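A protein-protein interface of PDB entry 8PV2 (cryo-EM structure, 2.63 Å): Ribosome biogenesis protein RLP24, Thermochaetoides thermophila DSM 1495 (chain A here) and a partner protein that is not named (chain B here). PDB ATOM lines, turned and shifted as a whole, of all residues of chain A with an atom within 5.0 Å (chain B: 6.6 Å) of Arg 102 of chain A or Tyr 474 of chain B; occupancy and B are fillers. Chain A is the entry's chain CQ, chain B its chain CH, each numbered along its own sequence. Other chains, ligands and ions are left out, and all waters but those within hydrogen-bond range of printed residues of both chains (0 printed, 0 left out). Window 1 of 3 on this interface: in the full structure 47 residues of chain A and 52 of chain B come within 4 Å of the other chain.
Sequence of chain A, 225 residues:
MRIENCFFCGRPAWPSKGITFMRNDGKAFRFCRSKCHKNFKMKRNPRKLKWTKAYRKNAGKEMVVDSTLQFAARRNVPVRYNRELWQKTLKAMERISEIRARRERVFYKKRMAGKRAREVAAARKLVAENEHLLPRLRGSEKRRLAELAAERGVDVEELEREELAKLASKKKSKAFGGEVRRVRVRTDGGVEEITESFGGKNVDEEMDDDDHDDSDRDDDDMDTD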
ATOM      1  N   ARG A  95      -5.399   4.039   8.030  1.00  0.00           N
ATOM      2  CA  ARG A  95      -4.895   2.666   8.013  1.00  0.00           C
ATOM      3  C   ARG A  95      -4.251   2.320   6.670  1.00  0.00           C
ATOM      4  O   ARG A  95      -3.197   1.665   6.624  1.00  0.00           O
ATOM      5  CB  ARG A  95      -6.027   1.696   8.344  1.00  0.00           C
ATOM      6  CG  ARG A  95      -5.589   0.255   8.382  1.00  0.00           C
ATOM      7  CD  ARG A  95      -4.632   0.040   9.531  1.00  0.00           C
ATOM      8  NE  ARG A  95      -4.209  -1.348   9.648  1.00  0.00           N
ATOM      9  CZ  ARG A  95      -3.252  -1.767  10.463  1.00  0.00           C
ATOM     10  NH1 ARG A  95      -2.580  -0.925  11.229  1.00  0.00           N
ATOM     11  NH2 ARG A  95      -2.960  -3.063  10.507  1.00  0.00           N
ATOM     12  N   GLU A  98      -0.723   3.857   6.491  1.00  0.00           N
ATOM     13  CA  GLU A  98       0.300   3.101   7.221  1.00  0.00           C
ATOM     14  C   GLU A  98       0.697   1.824   6.479  1.00  0.00           C
ATOM     15  O   GLU A  98       1.895   1.523   6.323  1.00  0.00           O
ATOM     16  CB  GLU A  98      -0.186   2.768   8.629  1.00  0.00           C
ATOM     17  CG  GLU A  98      -0.640   3.962   9.435  1.00  0.00           C
ATOM     18  CD  GLU A  98      -1.443   3.560  10.655  1.00  0.00           C
ATOM     19  OE1 GLU A  98      -1.276   2.414  11.122  1.00  0.00           O
ATOM     20  OE2 GLU A  98      -2.240   4.387  11.148  1.00  0.00           O
ATOM     21  N   ILE A  99      -0.299   1.074   5.994  1.00  0.00           N
ATOM     22  CA  ILE A  99      -0.022  -0.184   5.299  1.00  0.00           C
ATOM     23  C   ILE A  99       0.762   0.069   4.015  1.00  0.00           C
ATOM     24  O   ILE A  99       1.721  -0.655   3.698  1.00  0.00           O
ATOM     25  CB  ILE A  99      -1.339  -0.936   5.036  1.00  0.00           C
ATOM     26  CG1 ILE A  99      -1.959  -1.377   6.359  1.00  0.00           C
ATOM     27  CG2 ILE A  99      -1.116  -2.128   4.141  1.00  0.00           C
ATOM     28  CD1 ILE A  99      -3.313  -2.003   6.219  1.00  0.00           C
ATOM     29  N   ARG A 100       0.391   1.121   3.278  1.00  0.00           N
ATOM     30  CA  ARG A 100       1.102   1.491   2.061  1.00  0.00           C
ATOM     31  C   ARG A 100       2.549   1.860   2.347  1.00  0.00           C
ATOM     32  O   ARG A 100       3.444   1.509   1.570  1.00  0.00           O
ATOM     33  CB  ARG A 100       0.382   2.653   1.381  1.00  0.00           C
ATOM     34  CG  ARG A 100       0.981   3.070   0.058  1.00  0.00           C
ATOM     35  CD  ARG A 100       0.168   4.168  -0.586  1.00  0.00           C
ATOM     36  NE  ARG A 100       0.757   4.607  -1.844  1.00  0.00           N
ATOM     37  CZ  ARG A 100       0.242   5.547  -2.625  1.00  0.00           C
ATOM     38  NH1 ARG A 100      -0.883   6.166  -2.311  1.00  0.00           N
ATOM     39  NH2 ARG A 100       0.869   5.869  -3.752  1.00  0.00           N
ATOM     40  N   ALA A 101       2.800   2.564   3.456  1.00  0.00           N
ATOM     41  CA  ALA A 101       4.172   2.934   3.798  1.00  0.00           C
ATOM     42  C   ALA A 101       5.041   1.706   4.063  1.00  0.00           C
ATOM     43  O   ALA A 101       6.171   1.612   3.554  1.00  0.00           O
ATOM     44  CB  ALA A 101       4.175   3.862   5.009  1.00  0.00           C
ATOM     45  N   ARG A 102       4.527   0.746   4.842  1.00  0.00           N
ATOM     46  CA  ARG A 102       5.324  -0.452   5.123  1.00  0.00           C
ATOM     47  C   ARG A 102       5.561  -1.287   3.866  1.00  0.00           C
ATOM     48  O   ARG A 102       6.669  -1.807   3.650  1.00  0.00           O
ATOM     49  CB  ARG A 102       4.682  -1.287   6.232  1.00  0.00           C
ATOM     50  CG  ARG A 102       4.140  -0.454   7.370  1.00  0.00           C
ATOM     51  CD  ARG A 102       3.979  -1.240   8.657  1.00  0.00           C
ATOM     52  NE  ARG A 102       3.394  -2.559   8.461  1.00  0.00           N
ATOM     53  CZ  ARG A 102       2.172  -2.893   8.847  1.00  0.00           C
ATOM     54  NH1 ARG A 102       1.363  -2.015   9.416  1.00  0.00           N
ATOM     55  NH2 ARG A 102       1.750  -4.140   8.663  1.00  0.00           N
ATOM     56  N   ARG A 103       4.544  -1.404   3.006  1.00  0.00           N
ATOM     57  CA  ARG A 103       4.727  -2.173   1.777  1.00  0.00           C
ATOM     58  C   ARG A 103       5.699  -1.486   0.823  1.00  0.00           C
ATOM     59  O   ARG A 103       6.466  -2.160   0.122  1.00  0.00           O
ATOM     60  CB  ARG A 103       3.383  -2.414   1.104  1.00  0.00           C
ATOM     61  CG  ARG A 103       2.483  -3.312   1.913  1.00  0.00           C
ATOM     62  CD  ARG A 103       1.249  -3.712   1.150  1.00  0.00           C
ATOM     63  NE  ARG A 103       0.412  -4.612   1.930  1.00  0.00           N
ATOM     64  CZ  ARG A 103      -0.741  -5.111   1.510  1.00  0.00           C
ATOM     65  NH1 ARG A 103      -1.222  -4.823   0.311  1.00  0.00           N
ATOM     66  NH2 ARG A 103      -1.432  -5.914   2.312  1.00  0.00           N
ATOM     67  N   GLU A 104       5.700  -0.151   0.800  1.00  0.00           N
ATOM     68  CA  GLU A 104       6.665   0.580  -0.012  1.00  0.00           C
ATOM     69  C   GLU A 104       8.089   0.344   0.471  1.00  0.00           C
ATOM     70  O   GLU A 104       9.013   0.202  -0.342  1.00  0.00           O
ATOM     71  CB  GLU A 104       6.333   2.072   0.005  1.00  0.00           C
ATOM     72  CG  GLU A 104       7.002   2.881  -1.093  1.00  0.00           C
ATOM     73  CD  GLU A 104       8.365   3.419  -0.685  1.00  0.00           C
ATOM     74  OE1 GLU A 104       8.526   3.803   0.492  1.00  0.00           O
ATOM     75  OE2 GLU A 104       9.275   3.449  -1.540  1.00  0.00           O
ATOM     76  N   ARG A 105       8.289   0.314   1.793  1.00  0.00           N
ATOM     77  CA  ARG A 105       9.627   0.049   2.319  1.00  0.00           C
ATOM     78  C   ARG A 105      10.101  -1.356   1.950  1.00  0.00           C
ATOM     79  O   ARG A 105      11.274  -1.553   1.591  1.00  0.00           O
ATOM     80  CB  ARG A 105       9.649   0.252   3.833  1.00  0.00           C
ATOM     81  CG  ARG A 105      10.944  -0.175   4.490  1.00  0.00           C
ATOM     82  CD  ARG A 105      11.065   0.388   5.882  1.00  0.00           C
ATOM     83  NE  ARG A 105      11.672   1.711   5.879  1.00  0.00           N
ATOM     84  CZ  ARG A 105      12.955   1.945   6.115  1.00  0.00           C
ATOM     85  NH1 ARG A 105      13.800   0.962   6.374  1.00  0.00           N
ATOM     86  NH2 ARG A 105      13.400   3.197   6.098  1.00  0.00           N
ATOM     87  N   VAL A 106       9.195  -2.338   2.009  1.00  0.00           N
ATOM     88  CA  VAL A 106       9.544  -3.699   1.594  1.00  0.00           C
ATOM     89  C   VAL A 106       9.923  -3.736   0.112  1.00  0.00           C
ATOM     90  O   VAL A 106      10.894  -4.402  -0.283  1.00  0.00           O
ATOM     91  CB  VAL A 106       8.387  -4.663   1.915  1.00  0.00           C
ATOM     92  CG1 VAL A 106       8.635  -6.028   1.318  1.00  0.00           C
ATOM     93  CG2 VAL A 106       8.209  -4.780   3.415  1.00  0.00           C
ATOM     94  N   GLU B 464      -5.531  -9.720   4.217  1.00  0.00           N
ATOM     95  CA  GLU B 464      -4.303  -9.852   3.439  1.00  0.00           C
ATOM     96  C   GLU B 464      -3.084  -9.452   4.261  1.00  0.00           C
ATOM     97  O   GLU B 464      -2.025 -10.082   4.162  1.00  0.00           O
ATOM     98  CB  GLU B 464      -4.402  -9.015   2.165  1.00  0.00           C
ATOM     99  CG  GLU B 464      -3.149  -9.020   1.308  1.00  0.00           C
ATOM    100  CD  GLU B 464      -3.250  -8.073   0.132  1.00  0.00           C
ATOM    101  OE1 GLU B 464      -4.254  -7.337   0.049  1.00  0.00           O
ATOM    102  OE2 GLU B 464      -2.326  -8.058  -0.706  1.00  0.00           O
ATOM    103  N   GLU B 465      -3.224  -8.425   5.100  1.00  0.00           N
ATOM    104  CA  GLU B 465      -2.100  -7.961   5.904  1.00  0.00           C
ATOM    105  C   GLU B 465      -1.698  -8.991   6.951  1.00  0.00           C
ATOM    106  O   GLU B 465      -0.505  -9.249   7.155  1.00  0.00           O
ATOM    107  CB  GLU B 465      -2.448  -6.625   6.560  1.00  0.00           C
ATOM    108  CG  GLU B 465      -1.272  -5.933   7.222  1.00  0.00           C
ATOM    109  CD  GLU B 465      -0.346  -5.252   6.227  1.00  0.00           C
ATOM    110  OE1 GLU B 465      -0.648  -5.247   5.013  1.00  0.00           O
ATOM    111  OE2 GLU B 465       0.693  -4.716   6.659  1.00  0.00           O
ATOM    112  N   LEU B 468       0.046 -11.830   5.218  1.00  0.00           N
ATOM    113  CA  LEU B 468       1.424 -11.513   4.857  1.00  0.00           C
ATOM    114  C   LEU B 468       2.333 -11.499   6.080  1.00  0.00           C
ATOM    115  O   LEU B 468       3.491 -11.929   6.003  1.00  0.00           O
ATOM    116  CB  LEU B 468       1.475 -10.172   4.129  1.00  0.00           C
ATOM    117  CG  LEU B 468       0.935 -10.180   2.700  1.00  0.00           C
ATOM    118  CD1 LEU B 468       0.941  -8.779   2.117  1.00  0.00           C
ATOM    119  CD2 LEU B 468       1.729 -11.133   1.827  1.00  0.00           C
ATOM    120  N   GLU B 469       1.829 -11.012   7.218  1.00  0.00           N
ATOM    121  CA  GLU B 469       2.618 -11.058   8.448  1.00  0.00           C
ATOM    122  C   GLU B 469       2.853 -12.493   8.901  1.00  0.00           C
ATOM    123  O   GLU B 469       3.916 -12.811   9.448  1.00  0.00           O
ATOM    124  CB  GLU B 469       1.936 -10.261   9.558  1.00  0.00           C
ATOM    125  CG  GLU B 469       1.884  -8.767   9.324  1.00  0.00           C
ATOM    126  CD  GLU B 469       1.182  -8.037  10.450  1.00  0.00           C
ATOM    127  OE1 GLU B 469       0.631  -8.712  11.344  1.00  0.00           O
ATOM    128  OE2 GLU B 469       1.184  -6.787  10.445  1.00  0.00           O
ATOM    129  N   GLU B 471       3.056 -15.059   6.769  1.00  0.00           N
ATOM    130  CA  GLU B 471       4.020 -15.601   5.816  1.00  0.00           C
ATOM    131  C   GLU B 471       5.398 -14.964   5.920  1.00  0.00           C
ATOM    132  O   GLU B 471       6.332 -15.458   5.279  1.00  0.00           O
ATOM    133  CB  GLU B 471       3.507 -15.450   4.384  1.00  0.00           C
ATOM    134  CG  GLU B 471       2.248 -16.234   4.080  1.00  0.00           C
ATOM    135  CD  GLU B 471       1.621 -15.829   2.763  1.00  0.00           C
ATOM    136  OE1 GLU B 471       1.978 -14.752   2.241  1.00  0.00           O
ATOM    137  OE2 GLU B 471       0.771 -16.586   2.248  1.00  0.00           O
ATOM    138  N   GLY B 472       5.557 -13.889   6.688  1.00  0.00           N
ATOM    139  CA  GLY B 472       6.868 -13.285   6.817  1.00  0.00           C
ATOM    140  C   GLY B 472       7.206 -12.285   5.740  1.00  0.00           C
ATOM    141  O   GLY B 472       8.368 -12.189   5.339  1.00  0.00           O
ATOM    142  N   PHE B 473       6.209 -11.548   5.247  1.00  0.00           N
ATOM    143  CA  PHE B 473       6.450 -10.516   4.245  1.00  0.00           C
ATOM    144  C   PHE B 473       7.277  -9.372   4.817  1.00  0.00           C
ATOM    145  O   PHE B 473       8.143  -8.818   4.131  1.00  0.00           O
ATOM    146  CB  PHE B 473       5.112 -10.004   3.719  1.00  0.00           C
ATOM    147  CG  PHE B 473       5.209  -9.206   2.453  1.00  0.00           C
ATOM    148  CD1 PHE B 473       5.002  -7.840   2.470  1.00  0.00           C
ATOM    149  CD2 PHE B 473       5.472  -9.825   1.246  1.00  0.00           C
ATOM    150  CE1 PHE B 473       5.073  -7.101   1.311  1.00  0.00           C
ATOM    151  CE2 PHE B 473       5.545  -9.090   0.081  1.00  0.00           C
ATOM    152  CZ  PHE B 473       5.345  -7.727   0.113  1.00  0.00           C
ATOM    153  N   TYR B 474       7.032  -9.010   6.072  1.00  0.00           N
ATOM    154  CA  TYR B 474       7.675  -7.865   6.698  1.00  0.00           C
ATOM    155  C   TYR B 474       8.845  -8.256   7.591  1.00  0.00           C
ATOM    156  O   TYR B 474       9.338  -7.412   8.346  1.00  0.00           O
ATOM    157  CB  TYR B 474       6.653  -7.064   7.510  1.00  0.00           C
ATOM    158  CG  TYR B 474       5.464  -6.597   6.704  1.00  0.00           C
ATOM    159  CD1 TYR B 474       5.505  -5.400   6.002  1.00  0.00           C
ATOM    160  CD2 TYR B 474       4.302  -7.352   6.644  1.00  0.00           C
ATOM    161  CE1 TYR B 474       4.423  -4.971   5.264  1.00  0.00           C
ATOM    162  CE2 TYR B 474       3.217  -6.932   5.907  1.00  0.00           C
ATOM    163  CZ  TYR B 474       3.283  -5.742   5.220  1.00  0.00           C
ATOM    164  OH  TYR B 474       2.202  -5.323   4.488  1.00  0.00           O
ATOM    165  N   ASP B 475       9.294  -9.506   7.527  1.00  0.00           N
ATOM    166  CA  ASP B 475      10.384  -9.972   8.374  1.00  0.00           C
ATOM    167  C   ASP B 475      11.705  -9.400   7.875  1.00  0.00           C
ATOM    168  O   ASP B 475      12.028  -9.509   6.688  1.00  0.00           O
ATOM    169  CB  ASP B 475      10.434 -11.498   8.387  1.00  0.00           C
ATOM    170  CG  ASP B 475       9.328 -12.106   9.221  1.00  0.00           C
ATOM    171  OD1 ASP B 475       8.395 -11.369   9.600  1.00  0.00           O
ATOM    172  OD2 ASP B 475       9.391 -13.323   9.496  1.00  0.00           O
ATOM    173  N   GLU B 476      12.468  -8.799   8.781  1.00  0.00           N
ATOM    174  CA  GLU B 476      13.757  -8.205   8.455  1.00  0.00           C
ATOM    175  C   GLU B 476      14.867  -9.153   8.887  1.00  0.00           C
ATOM    176  O   GLU B 476      14.740  -9.841   9.905  1.00  0.00           O
ATOM    177  CB  GLU B 476      13.915  -6.845   9.138  1.00  0.00           C
ATOM    178  CG  GLU B 476      15.025  -5.971   8.568  1.00  0.00           C
ATOM    179  CD  GLU B 476      16.367  -6.209   9.238  1.00  0.00           C
ATOM    180  OE1 GLU B 476      16.381  -6.588  10.427  1.00  0.00           O
ATOM    181  OE2 GLU B 476      17.406  -6.018   8.572  1.00  0.00           O
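The guanidinium group (NE) of Arg 102 of chain A is in salt-bridge range of the side-chain carboxylate (OE2) of Glu 465 of chain B, 3.9 Å away.
The side-chain carboxylate of Glu 469 of chain B lies within salt-bridge range of the guanidinium group of Arg 102 of chain A, 3.2 Å away.
The guanidinium group (NH1) of Arg 103 of chain A is in salt-bridge range of the side-chain carboxylate (OE2) of Glu 464 of chain B.
NH2 of Arg 103 of chain A is in salt-bridge range of OE1 of Glu 465 of chain B (2.9 Å).
NE of Arg 103 of chain A sits at hydrogen-bond distance from OH of Tyr 474 of chain B (3.2 Å).
The side-chain carboxylate (OE2) of Glu 465 of chain B lies within hydrogen-bond range of the side-chain hydroxyl (OH) of Tyr 474 of chain B (2.7 Å).
The backbone carbonyl oxygen of Leu 468 of chain B sits at hydrogen-bond distance from the backbone NH of Phe 473 of chain B.
Among the printed residues, pairs that only touch across the chains: Ile 99 of chain A with Glu 465 of chain B (3.3 Å), Val 106 of chain A with Phe 473 of chain B (3.7 Å), Arg 103 of chain A with Leu 468 of chain B (3.7 Å), Val 106 of chain A with Tyr 474 of chain B (3.8 Å) and Arg 102 of chain A with Tyr 474 of chain B (3.8 Å).
Printed residues of chain B within 4 Å of Arg 102 of chain A: Glu 465, Glu 469 and Tyr 474.
Tyr 474 of chain B touches three residues of chain A.
Printed residues of chain A within 4 Å of Glu 469 of chain B: Arg 102.
Of the printed residues of chain B, Val 106 of chain A touches Phe 473 and Tyr 474.
The nearest residue of chain A that does not touch Tyr 474 of chain B is Ile 99 of chain A (4.6 Å).
The nearest printed residue of chain B that does not touch Val 106 of chain A is Asp 475 of chain B (6.4 Å).
Printed residues of chain A that touch a printed residue of chain B: Ile 99, Arg 102, Arg 103 and Val 106.
Printed residues of chain B that touch a printed residue of chain A: Glu 464, Glu 465, Leu 468, Glu 469, Phe 473 and Tyr 474.
Among the printed residues, 10 pairs touch across the chains.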
